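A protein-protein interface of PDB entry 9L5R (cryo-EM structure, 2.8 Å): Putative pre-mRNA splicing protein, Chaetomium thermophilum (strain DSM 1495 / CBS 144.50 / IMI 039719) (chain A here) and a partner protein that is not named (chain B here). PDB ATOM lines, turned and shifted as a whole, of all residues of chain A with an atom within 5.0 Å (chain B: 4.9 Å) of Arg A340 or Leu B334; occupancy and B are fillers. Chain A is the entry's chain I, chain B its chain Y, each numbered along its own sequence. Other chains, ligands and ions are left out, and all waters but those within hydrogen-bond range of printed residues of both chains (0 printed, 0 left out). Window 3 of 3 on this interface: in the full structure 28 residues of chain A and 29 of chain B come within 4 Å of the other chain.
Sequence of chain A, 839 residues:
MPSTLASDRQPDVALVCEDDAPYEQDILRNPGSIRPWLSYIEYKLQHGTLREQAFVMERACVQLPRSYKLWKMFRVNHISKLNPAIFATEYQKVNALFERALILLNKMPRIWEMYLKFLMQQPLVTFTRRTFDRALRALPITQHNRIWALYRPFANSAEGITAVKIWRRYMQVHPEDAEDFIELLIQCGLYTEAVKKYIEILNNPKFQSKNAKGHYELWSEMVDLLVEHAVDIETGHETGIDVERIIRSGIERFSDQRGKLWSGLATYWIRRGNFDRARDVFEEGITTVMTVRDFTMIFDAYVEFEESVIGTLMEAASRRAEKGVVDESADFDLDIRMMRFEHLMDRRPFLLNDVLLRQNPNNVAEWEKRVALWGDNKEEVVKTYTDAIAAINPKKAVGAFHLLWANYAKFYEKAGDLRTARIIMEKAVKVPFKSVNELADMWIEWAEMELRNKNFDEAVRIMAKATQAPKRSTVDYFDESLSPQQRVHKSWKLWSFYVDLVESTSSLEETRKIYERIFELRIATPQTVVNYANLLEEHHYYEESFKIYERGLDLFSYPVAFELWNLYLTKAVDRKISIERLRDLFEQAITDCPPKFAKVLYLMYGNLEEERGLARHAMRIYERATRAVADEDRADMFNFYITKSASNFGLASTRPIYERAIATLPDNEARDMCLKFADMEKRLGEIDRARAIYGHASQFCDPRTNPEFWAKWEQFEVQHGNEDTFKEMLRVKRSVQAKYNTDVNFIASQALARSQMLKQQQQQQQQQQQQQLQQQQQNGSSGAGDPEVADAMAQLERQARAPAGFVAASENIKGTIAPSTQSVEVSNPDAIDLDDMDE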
ATOM      1  N   ARG A 279     -12.042 -30.955 -23.189  1.00  0.00           N
ATOM      2  CA  ARG A 279     -12.956 -30.185 -24.030  1.00  0.00           C
ATOM      3  C   ARG A 279     -12.853 -30.594 -25.497  1.00  0.00           C
ATOM      4  O   ARG A 279     -13.862 -30.621 -26.209  1.00  0.00           O
ATOM      5  CB  ARG A 279     -12.677 -28.690 -23.872  1.00  0.00           C
ATOM      6  CG  ARG A 279     -13.228 -28.088 -22.590  1.00  0.00           C
ATOM      7  CD  ARG A 279     -12.911 -26.605 -22.505  1.00  0.00           C
ATOM      8  NE  ARG A 279     -13.473 -25.992 -21.307  1.00  0.00           N
ATOM      9  CZ  ARG A 279     -12.855 -25.939 -20.136  1.00  0.00           C
ATOM     10  NH1 ARG A 279     -11.658 -26.476 -19.961  1.00  0.00           N
ATOM     11  NH2 ARG A 279     -13.453 -25.335 -19.113  1.00  0.00           N
ATOM     12  N   ILE A 336     -13.665 -14.755 -21.002  1.00  0.00           N
ATOM     13  CA  ILE A 336     -13.643 -15.623 -22.175  1.00  0.00           C
ATOM     14  C   ILE A 336     -14.238 -17.000 -21.882  1.00  0.00           C
ATOM     15  O   ILE A 336     -14.811 -17.617 -22.790  1.00  0.00           O
ATOM     16  CB  ILE A 336     -12.223 -15.733 -22.771  1.00  0.00           C
ATOM     17  CG1 ILE A 336     -11.275 -16.493 -21.843  1.00  0.00           C
ATOM     18  CG2 ILE A 336     -11.689 -14.345 -23.069  1.00  0.00           C
ATOM     19  CD1 ILE A 336     -10.051 -17.067 -22.517  1.00  0.00           C
ATOM     20  N   ARG A 337     -14.155 -17.495 -20.638  1.00  0.00           N
ATOM     21  CA  ARG A 337     -14.826 -18.751 -20.303  1.00  0.00           C
ATOM     22  C   ARG A 337     -16.337 -18.602 -20.388  1.00  0.00           C
ATOM     23  O   ARG A 337     -17.023 -19.471 -20.938  1.00  0.00           O
ATOM     24  CB  ARG A 337     -14.432 -19.230 -18.906  1.00  0.00           C
ATOM     25  CG  ARG A 337     -12.991 -19.649 -18.762  1.00  0.00           C
ATOM     26  CD  ARG A 337     -12.696 -20.137 -17.360  1.00  0.00           C
ATOM     27  NE  ARG A 337     -11.280 -20.439 -17.206  1.00  0.00           N
ATOM     28  CZ  ARG A 337     -10.718 -21.609 -17.465  1.00  0.00           C
ATOM     29  NH1 ARG A 337     -11.430 -22.640 -17.888  1.00  0.00           N
ATOM     30  NH2 ARG A 337      -9.406 -21.743 -17.307  1.00  0.00           N
ATOM     31  N   MET A 338     -16.879 -17.504 -19.853  1.00  0.00           N
ATOM     32  CA  MET A 338     -18.320 -17.298 -19.965  1.00  0.00           C
ATOM     33  C   MET A 338     -18.746 -16.986 -21.392  1.00  0.00           C
ATOM     34  O   MET A 338     -19.860 -17.346 -21.783  1.00  0.00           O
ATOM     35  CB  MET A 338     -18.789 -16.208 -19.006  1.00  0.00           C
ATOM     36  CG  MET A 338     -18.882 -16.709 -17.589  1.00  0.00           C
ATOM     37  SD  MET A 338     -19.703 -15.576 -16.469  1.00  0.00           S
ATOM     38  CE  MET A 338     -19.365 -16.420 -14.936  1.00  0.00           C
ATOM     39  N   MET A 339     -17.880 -16.349 -22.185  1.00  0.00           N
ATOM     40  CA  MET A 339     -18.146 -16.205 -23.615  1.00  0.00           C
ATOM     41  C   MET A 339     -18.271 -17.570 -24.281  1.00  0.00           C
ATOM     42  O   MET A 339     -19.238 -17.832 -25.014  1.00  0.00           O
ATOM     43  CB  MET A 339     -17.033 -15.365 -24.255  1.00  0.00           C
ATOM     44  CG  MET A 339     -17.167 -15.047 -25.750  1.00  0.00           C
ATOM     45  SD  MET A 339     -16.621 -16.333 -26.899  1.00  0.00           S
ATOM     46  CE  MET A 339     -14.844 -16.237 -26.700  1.00  0.00           C
ATOM     47  N   ARG A 340     -17.313 -18.462 -24.005  1.00  0.00           N
ATOM     48  CA  ARG A 340     -17.344 -19.809 -24.566  1.00  0.00           C
ATOM     49  C   ARG A 340     -18.595 -20.559 -24.131  1.00  0.00           C
ATOM     50  O   ARG A 340     -19.271 -21.187 -24.952  1.00  0.00           O
ATOM     51  CB  ARG A 340     -16.090 -20.581 -24.152  1.00  0.00           C
ATOM     52  CG  ARG A 340     -14.825 -20.203 -24.903  1.00  0.00           C
ATOM     53  CD  ARG A 340     -13.592 -20.583 -24.097  1.00  0.00           C
ATOM     54  NE  ARG A 340     -12.417 -20.781 -24.938  1.00  0.00           N
ATOM     55  CZ  ARG A 340     -11.588 -21.811 -24.833  1.00  0.00           C
ATOM     56  NH1 ARG A 340     -11.777 -22.761 -23.930  1.00  0.00           N
ATOM     57  NH2 ARG A 340     -10.545 -21.892 -25.652  1.00  0.00           N
ATOM     58  N   PHE A 341     -18.940 -20.468 -22.846  1.00  0.00           N
ATOM     59  CA  PHE A 341     -20.078 -21.225 -22.334  1.00  0.00           C
ATOM     60  C   PHE A 341     -21.393 -20.688 -22.880  1.00  0.00           C
ATOM     61  O   PHE A 341     -22.277 -21.471 -23.242  1.00  0.00           O
ATOM     62  CB  PHE A 341     -20.078 -21.212 -20.807  1.00  0.00           C
ATOM     63  CG  PHE A 341     -18.878 -21.875 -20.203  1.00  0.00           C
ATOM     64  CD1 PHE A 341     -18.211 -22.885 -20.882  1.00  0.00           C
ATOM     65  CD2 PHE A 341     -18.408 -21.485 -18.965  1.00  0.00           C
ATOM     66  CE1 PHE A 341     -17.102 -23.489 -20.335  1.00  0.00           C
ATOM     67  CE2 PHE A 341     -17.300 -22.086 -18.418  1.00  0.00           C
ATOM     68  CZ  PHE A 341     -16.647 -23.086 -19.100  1.00  0.00           C
ATOM     69  N   GLU A 342     -21.527 -19.362 -22.990  1.00  0.00           N
ATOM     70  CA  GLU A 342     -22.755 -18.785 -23.525  1.00  0.00           C
ATOM     71  C   GLU A 342     -22.939 -19.124 -25.000  1.00  0.00           C
ATOM     72  O   GLU A 342     -24.036 -19.519 -25.410  1.00  0.00           O
ATOM     73  CB  GLU A 342     -22.764 -17.271 -23.314  1.00  0.00           C
ATOM     74  CG  GLU A 342     -23.051 -16.849 -21.882  1.00  0.00           C
ATOM     75  CD  GLU A 342     -24.478 -17.137 -21.461  1.00  0.00           C
ATOM     76  OE1 GLU A 342     -25.379 -17.076 -22.323  1.00  0.00           O
ATOM     77  OE2 GLU A 342     -24.699 -17.426 -20.266  1.00  0.00           O
ATOM     78  N   HIS A 343     -21.881 -19.011 -25.811  1.00  0.00           N
ATOM     79  CA  HIS A 343     -22.064 -19.304 -27.231  1.00  0.00           C
ATOM     80  C   HIS A 343     -22.208 -20.801 -27.499  1.00  0.00           C
ATOM     81  O   HIS A 343     -22.984 -21.197 -28.377  1.00  0.00           O
ATOM     82  CB  HIS A 343     -20.942 -18.697 -28.070  1.00  0.00           C
ATOM     83  CG  HIS A 343     -20.914 -17.200 -28.054  1.00  0.00           C
ATOM     84  ND1 HIS A 343     -21.821 -16.438 -28.760  1.00  0.00           N
ATOM     85  CD2 HIS A 343     -20.075 -16.324 -27.453  1.00  0.00           C
ATOM     86  CE1 HIS A 343     -21.556 -15.158 -28.575  1.00  0.00           C
ATOM     87  NE2 HIS A 343     -20.501 -15.061 -27.786  1.00  0.00           N
ATOM     88  N   LEU A 344     -21.504 -21.656 -26.748  1.00  0.00           N
ATOM     89  CA  LEU A 344     -21.733 -23.093 -26.891  1.00  0.00           C
ATOM     90  C   LEU A 344     -23.121 -23.496 -26.403  1.00  0.00           C
ATOM     91  O   LEU A 344     -23.743 -24.394 -26.978  1.00  0.00           O
ATOM     92  CB  LEU A 344     -20.650 -23.895 -26.167  1.00  0.00           C
ATOM     93  CG  LEU A 344     -19.409 -24.314 -26.970  1.00  0.00           C
ATOM     94  CD1 LEU A 344     -18.494 -23.166 -27.341  1.00  0.00           C
ATOM     95  CD2 LEU A 344     -18.633 -25.378 -26.202  1.00  0.00           C
ATOM     96  N   MET A 345     -23.644 -22.833 -25.372  1.00  0.00           N
ATOM     97  CA  MET A 345     -24.979 -23.179 -24.908  1.00  0.00           C
ATOM     98  C   MET A 345     -26.045 -22.664 -25.867  1.00  0.00           C
ATOM     99  O   MET A 345     -27.115 -23.272 -25.993  1.00  0.00           O
ATOM    100  CB  MET A 345     -25.192 -22.636 -23.496  1.00  0.00           C
ATOM    101  CG  MET A 345     -26.438 -23.152 -22.820  1.00  0.00           C
ATOM    102  SD  MET A 345     -26.513 -22.660 -21.096  1.00  0.00           S
ATOM    103  CE  MET A 345     -27.847 -23.701 -20.527  1.00  0.00           C
ATOM    104  N   ARG A 347     -25.432 -22.559 -29.119  1.00  0.00           N
ATOM    105  CA  ARG A 347     -25.277 -23.490 -30.231  1.00  0.00           C
ATOM    106  C   ARG A 347     -25.707 -24.909 -29.882  1.00  0.00           C
ATOM    107  O   ARG A 347     -25.748 -25.762 -30.776  1.00  0.00           O
ATOM    108  CB  ARG A 347     -23.820 -23.501 -30.701  1.00  0.00           C
ATOM    109  CG  ARG A 347     -23.417 -22.275 -31.500  1.00  0.00           C
ATOM    110  CD  ARG A 347     -22.150 -22.528 -32.302  1.00  0.00           C
ATOM    111  NE  ARG A 347     -20.998 -22.771 -31.442  1.00  0.00           N
ATOM    112  CZ  ARG A 347     -20.345 -23.922 -31.369  1.00  0.00           C
ATOM    113  NH1 ARG A 347     -20.705 -24.968 -32.095  1.00  0.00           N
ATOM    114  NH2 ARG A 347     -19.305 -24.028 -30.547  1.00  0.00           N
ATOM    115  N   GLN B 318      -4.994 -17.738 -30.064  1.00  0.00           N
ATOM    116  CA  GLN B 318      -6.356 -17.363 -29.703  1.00  0.00           C
ATOM    117  C   GLN B 318      -6.373 -16.106 -28.847  1.00  0.00           C
ATOM    118  O   GLN B 318      -7.273 -15.275 -28.994  1.00  0.00           O
ATOM    119  CB  GLN B 318      -7.076 -18.519 -28.997  1.00  0.00           C
ATOM    120  CG  GLN B 318      -6.433 -19.032 -27.720  1.00  0.00           C
ATOM    121  CD  GLN B 318      -7.087 -18.480 -26.468  1.00  0.00           C
ATOM    122  OE1 GLN B 318      -8.260 -18.109 -26.476  1.00  0.00           O
ATOM    123  NE2 GLN B 318      -6.331 -18.437 -25.378  1.00  0.00           N
ATOM    124  N   THR B 330     -14.599 -14.143 -32.695  1.00  0.00           N
ATOM    125  CA  THR B 330     -15.265 -14.782 -31.566  1.00  0.00           C
ATOM    126  C   THR B 330     -15.461 -16.269 -31.830  1.00  0.00           C
ATOM    127  O   THR B 330     -15.208 -17.100 -30.952  1.00  0.00           O
ATOM    128  CB  THR B 330     -16.609 -14.100 -31.297  1.00  0.00           C
ATOM    129  OG1 THR B 330     -16.394 -12.715 -30.999  1.00  0.00           O
ATOM    130  CG2 THR B 330     -17.326 -14.754 -30.126  1.00  0.00           C
ATOM    131  N   VAL B 331     -15.872 -16.619 -33.051  1.00  0.00           N
ATOM    132  CA  VAL B 331     -16.012 -18.022 -33.434  1.00  0.00           C
ATOM    133  C   VAL B 331     -14.656 -18.718 -33.453  1.00  0.00           C
ATOM    134  O   VAL B 331     -14.557 -19.905 -33.116  1.00  0.00           O
ATOM    135  CB  VAL B 331     -16.725 -18.124 -34.796  1.00  0.00           C
ATOM    136  CG1 VAL B 331     -17.128 -19.564 -35.089  1.00  0.00           C
ATOM    137  CG2 VAL B 331     -17.939 -17.209 -34.828  1.00  0.00           C
ATOM    138  N   LEU B 332     -13.594 -18.006 -33.843  1.00  0.00           N
ATOM    139  CA  LEU B 332     -12.254 -18.587 -33.803  1.00  0.00           C
ATOM    140  C   LEU B 332     -11.816 -18.872 -32.371  1.00  0.00           C
ATOM    141  O   LEU B 332     -11.176 -19.897 -32.105  1.00  0.00           O
ATOM    142  CB  LEU B 332     -11.259 -17.661 -34.505  1.00  0.00           C
ATOM    143  CG  LEU B 332      -9.851 -18.205 -34.775  1.00  0.00           C
ATOM    144  CD1 LEU B 332      -9.391 -17.814 -36.168  1.00  0.00           C
ATOM    145  CD2 LEU B 332      -8.853 -17.703 -33.740  1.00  0.00           C
ATOM    146  N   ALA B 333     -12.141 -17.974 -31.437  1.00  0.00           N
ATOM    147  CA  ALA B 333     -11.851 -18.234 -30.031  1.00  0.00           C
ATOM    148  C   ALA B 333     -12.705 -19.370 -29.484  1.00  0.00           C
ATOM    149  O   ALA B 333     -12.259 -20.112 -28.602  1.00  0.00           O
ATOM    150  CB  ALA B 333     -12.062 -16.964 -29.206  1.00  0.00           C
ATOM    151  N   LEU B 334     -13.937 -19.504 -29.982  1.00  0.00           N
ATOM    152  CA  LEU B 334     -14.786 -20.631 -29.607  1.00  0.00           C
ATOM    153  C   LEU B 334     -14.195 -21.949 -30.081  1.00  0.00           C
ATOM    154  O   LEU B 334     -14.209 -22.946 -29.348  1.00  0.00           O
ATOM    155  CB  LEU B 334     -16.182 -20.454 -30.199  1.00  0.00           C
ATOM    156  CG  LEU B 334     -17.053 -19.355 -29.607  1.00  0.00           C
ATOM    157  CD1 LEU B 334     -18.245 -19.085 -30.512  1.00  0.00           C
ATOM    158  CD2 LEU B 334     -17.479 -19.732 -28.217  1.00  0.00           C
ATOM    159  N   SER B 335     -13.685 -21.971 -31.310  1.00  0.00           N
ATOM    160  CA  SER B 335     -13.127 -23.176 -31.912  1.00  0.00           C
ATOM    161  C   SER B 335     -11.854 -23.564 -31.172  1.00  0.00           C
ATOM    162  O   SER B 335     -10.859 -22.834 -31.203  1.00  0.00           O
ATOM    163  CB  SER B 335     -12.858 -22.934 -33.393  1.00  0.00           C
ATOM    164  OG  SER B 335     -12.512 -24.133 -34.059  1.00  0.00           O
ATOM    165  N   ASN B 336     -11.886 -24.715 -30.505  1.00  0.00           N
ATOM    166  CA  ASN B 336     -10.790 -25.144 -29.649  1.00  0.00           C
ATOM    167  C   ASN B 336      -9.655 -25.716 -30.499  1.00  0.00           C
ATOM    168  O   ASN B 336      -9.671 -25.652 -31.731  1.00  0.00           O
ATOM    169  CB  ASN B 336     -11.295 -26.141 -28.611  1.00  0.00           C
ATOM    170  CG  ASN B 336     -12.246 -25.510 -27.614  1.00  0.00           C
ATOM    171  OD1 ASN B 336     -13.340 -26.018 -27.376  1.00  0.00           O
ATOM    172  ND2 ASN B 336     -11.832 -24.393 -27.027  1.00  0.00           N
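The side-chain amide nitrogen (ND2) of Asn B336 lies close to the guanidinium group (NH2) of Arg A340, 3.1 Å away.
Met A339 touches Thr B330.
CB of Ala B333 touches CE of Met A339, 3.8 Å away.
CD2 of Leu B334 touches SD of Met A339, at 3.7 Å.
NE of Arg A340 touches O of Ala B333, at 3.7 Å.
CA of Arg A340 touches CD2 of Leu B334, 3.7 Å away.
His A343 touches Thr B330 (NE2 to CG2, 3.96 Å).
CD2 of Leu B334 touches CB of His A343, at 3.6 Å.
Leu B334 touches Leu A344.
Of the printed residues of chain B, Arg A340 touches Ala B333, Leu B334 and Asn B336.
Leu B334 touches four residues of chain A.
Printed residues of chain B within 4 Å of Met A339: Thr B330, Ala B333 and Leu B334.
Printed residues of chain A within 4 Å of Ala B333: Met A339 and Arg A340.
Printed residues of chain B within 4 Å of His A343: Thr B330 and Leu B334.
Of the printed residues of chain A, Thr B330 touches Met A339 and His A343.
Of the printed residues of chain B, Leu A344 touches Leu B334 (3.7 Å).
Met A345 touches none of the printed residues of chain B.
The nearest residue of chain B that does not touch Arg A340 is Gln B318 (4.5 Å).
The nearest residue of chain A that does not touch Leu B334 is Arg A347 (4.7 Å).
Hydrophobic or aromatic side chains of chain A that line the printed part of chain B: Met A339, His A343 and Leu A344.
Hydrophobic or aromatic side chains of chain B within 4 Å of the printed part of chain A: Ala B333 and Leu B334.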
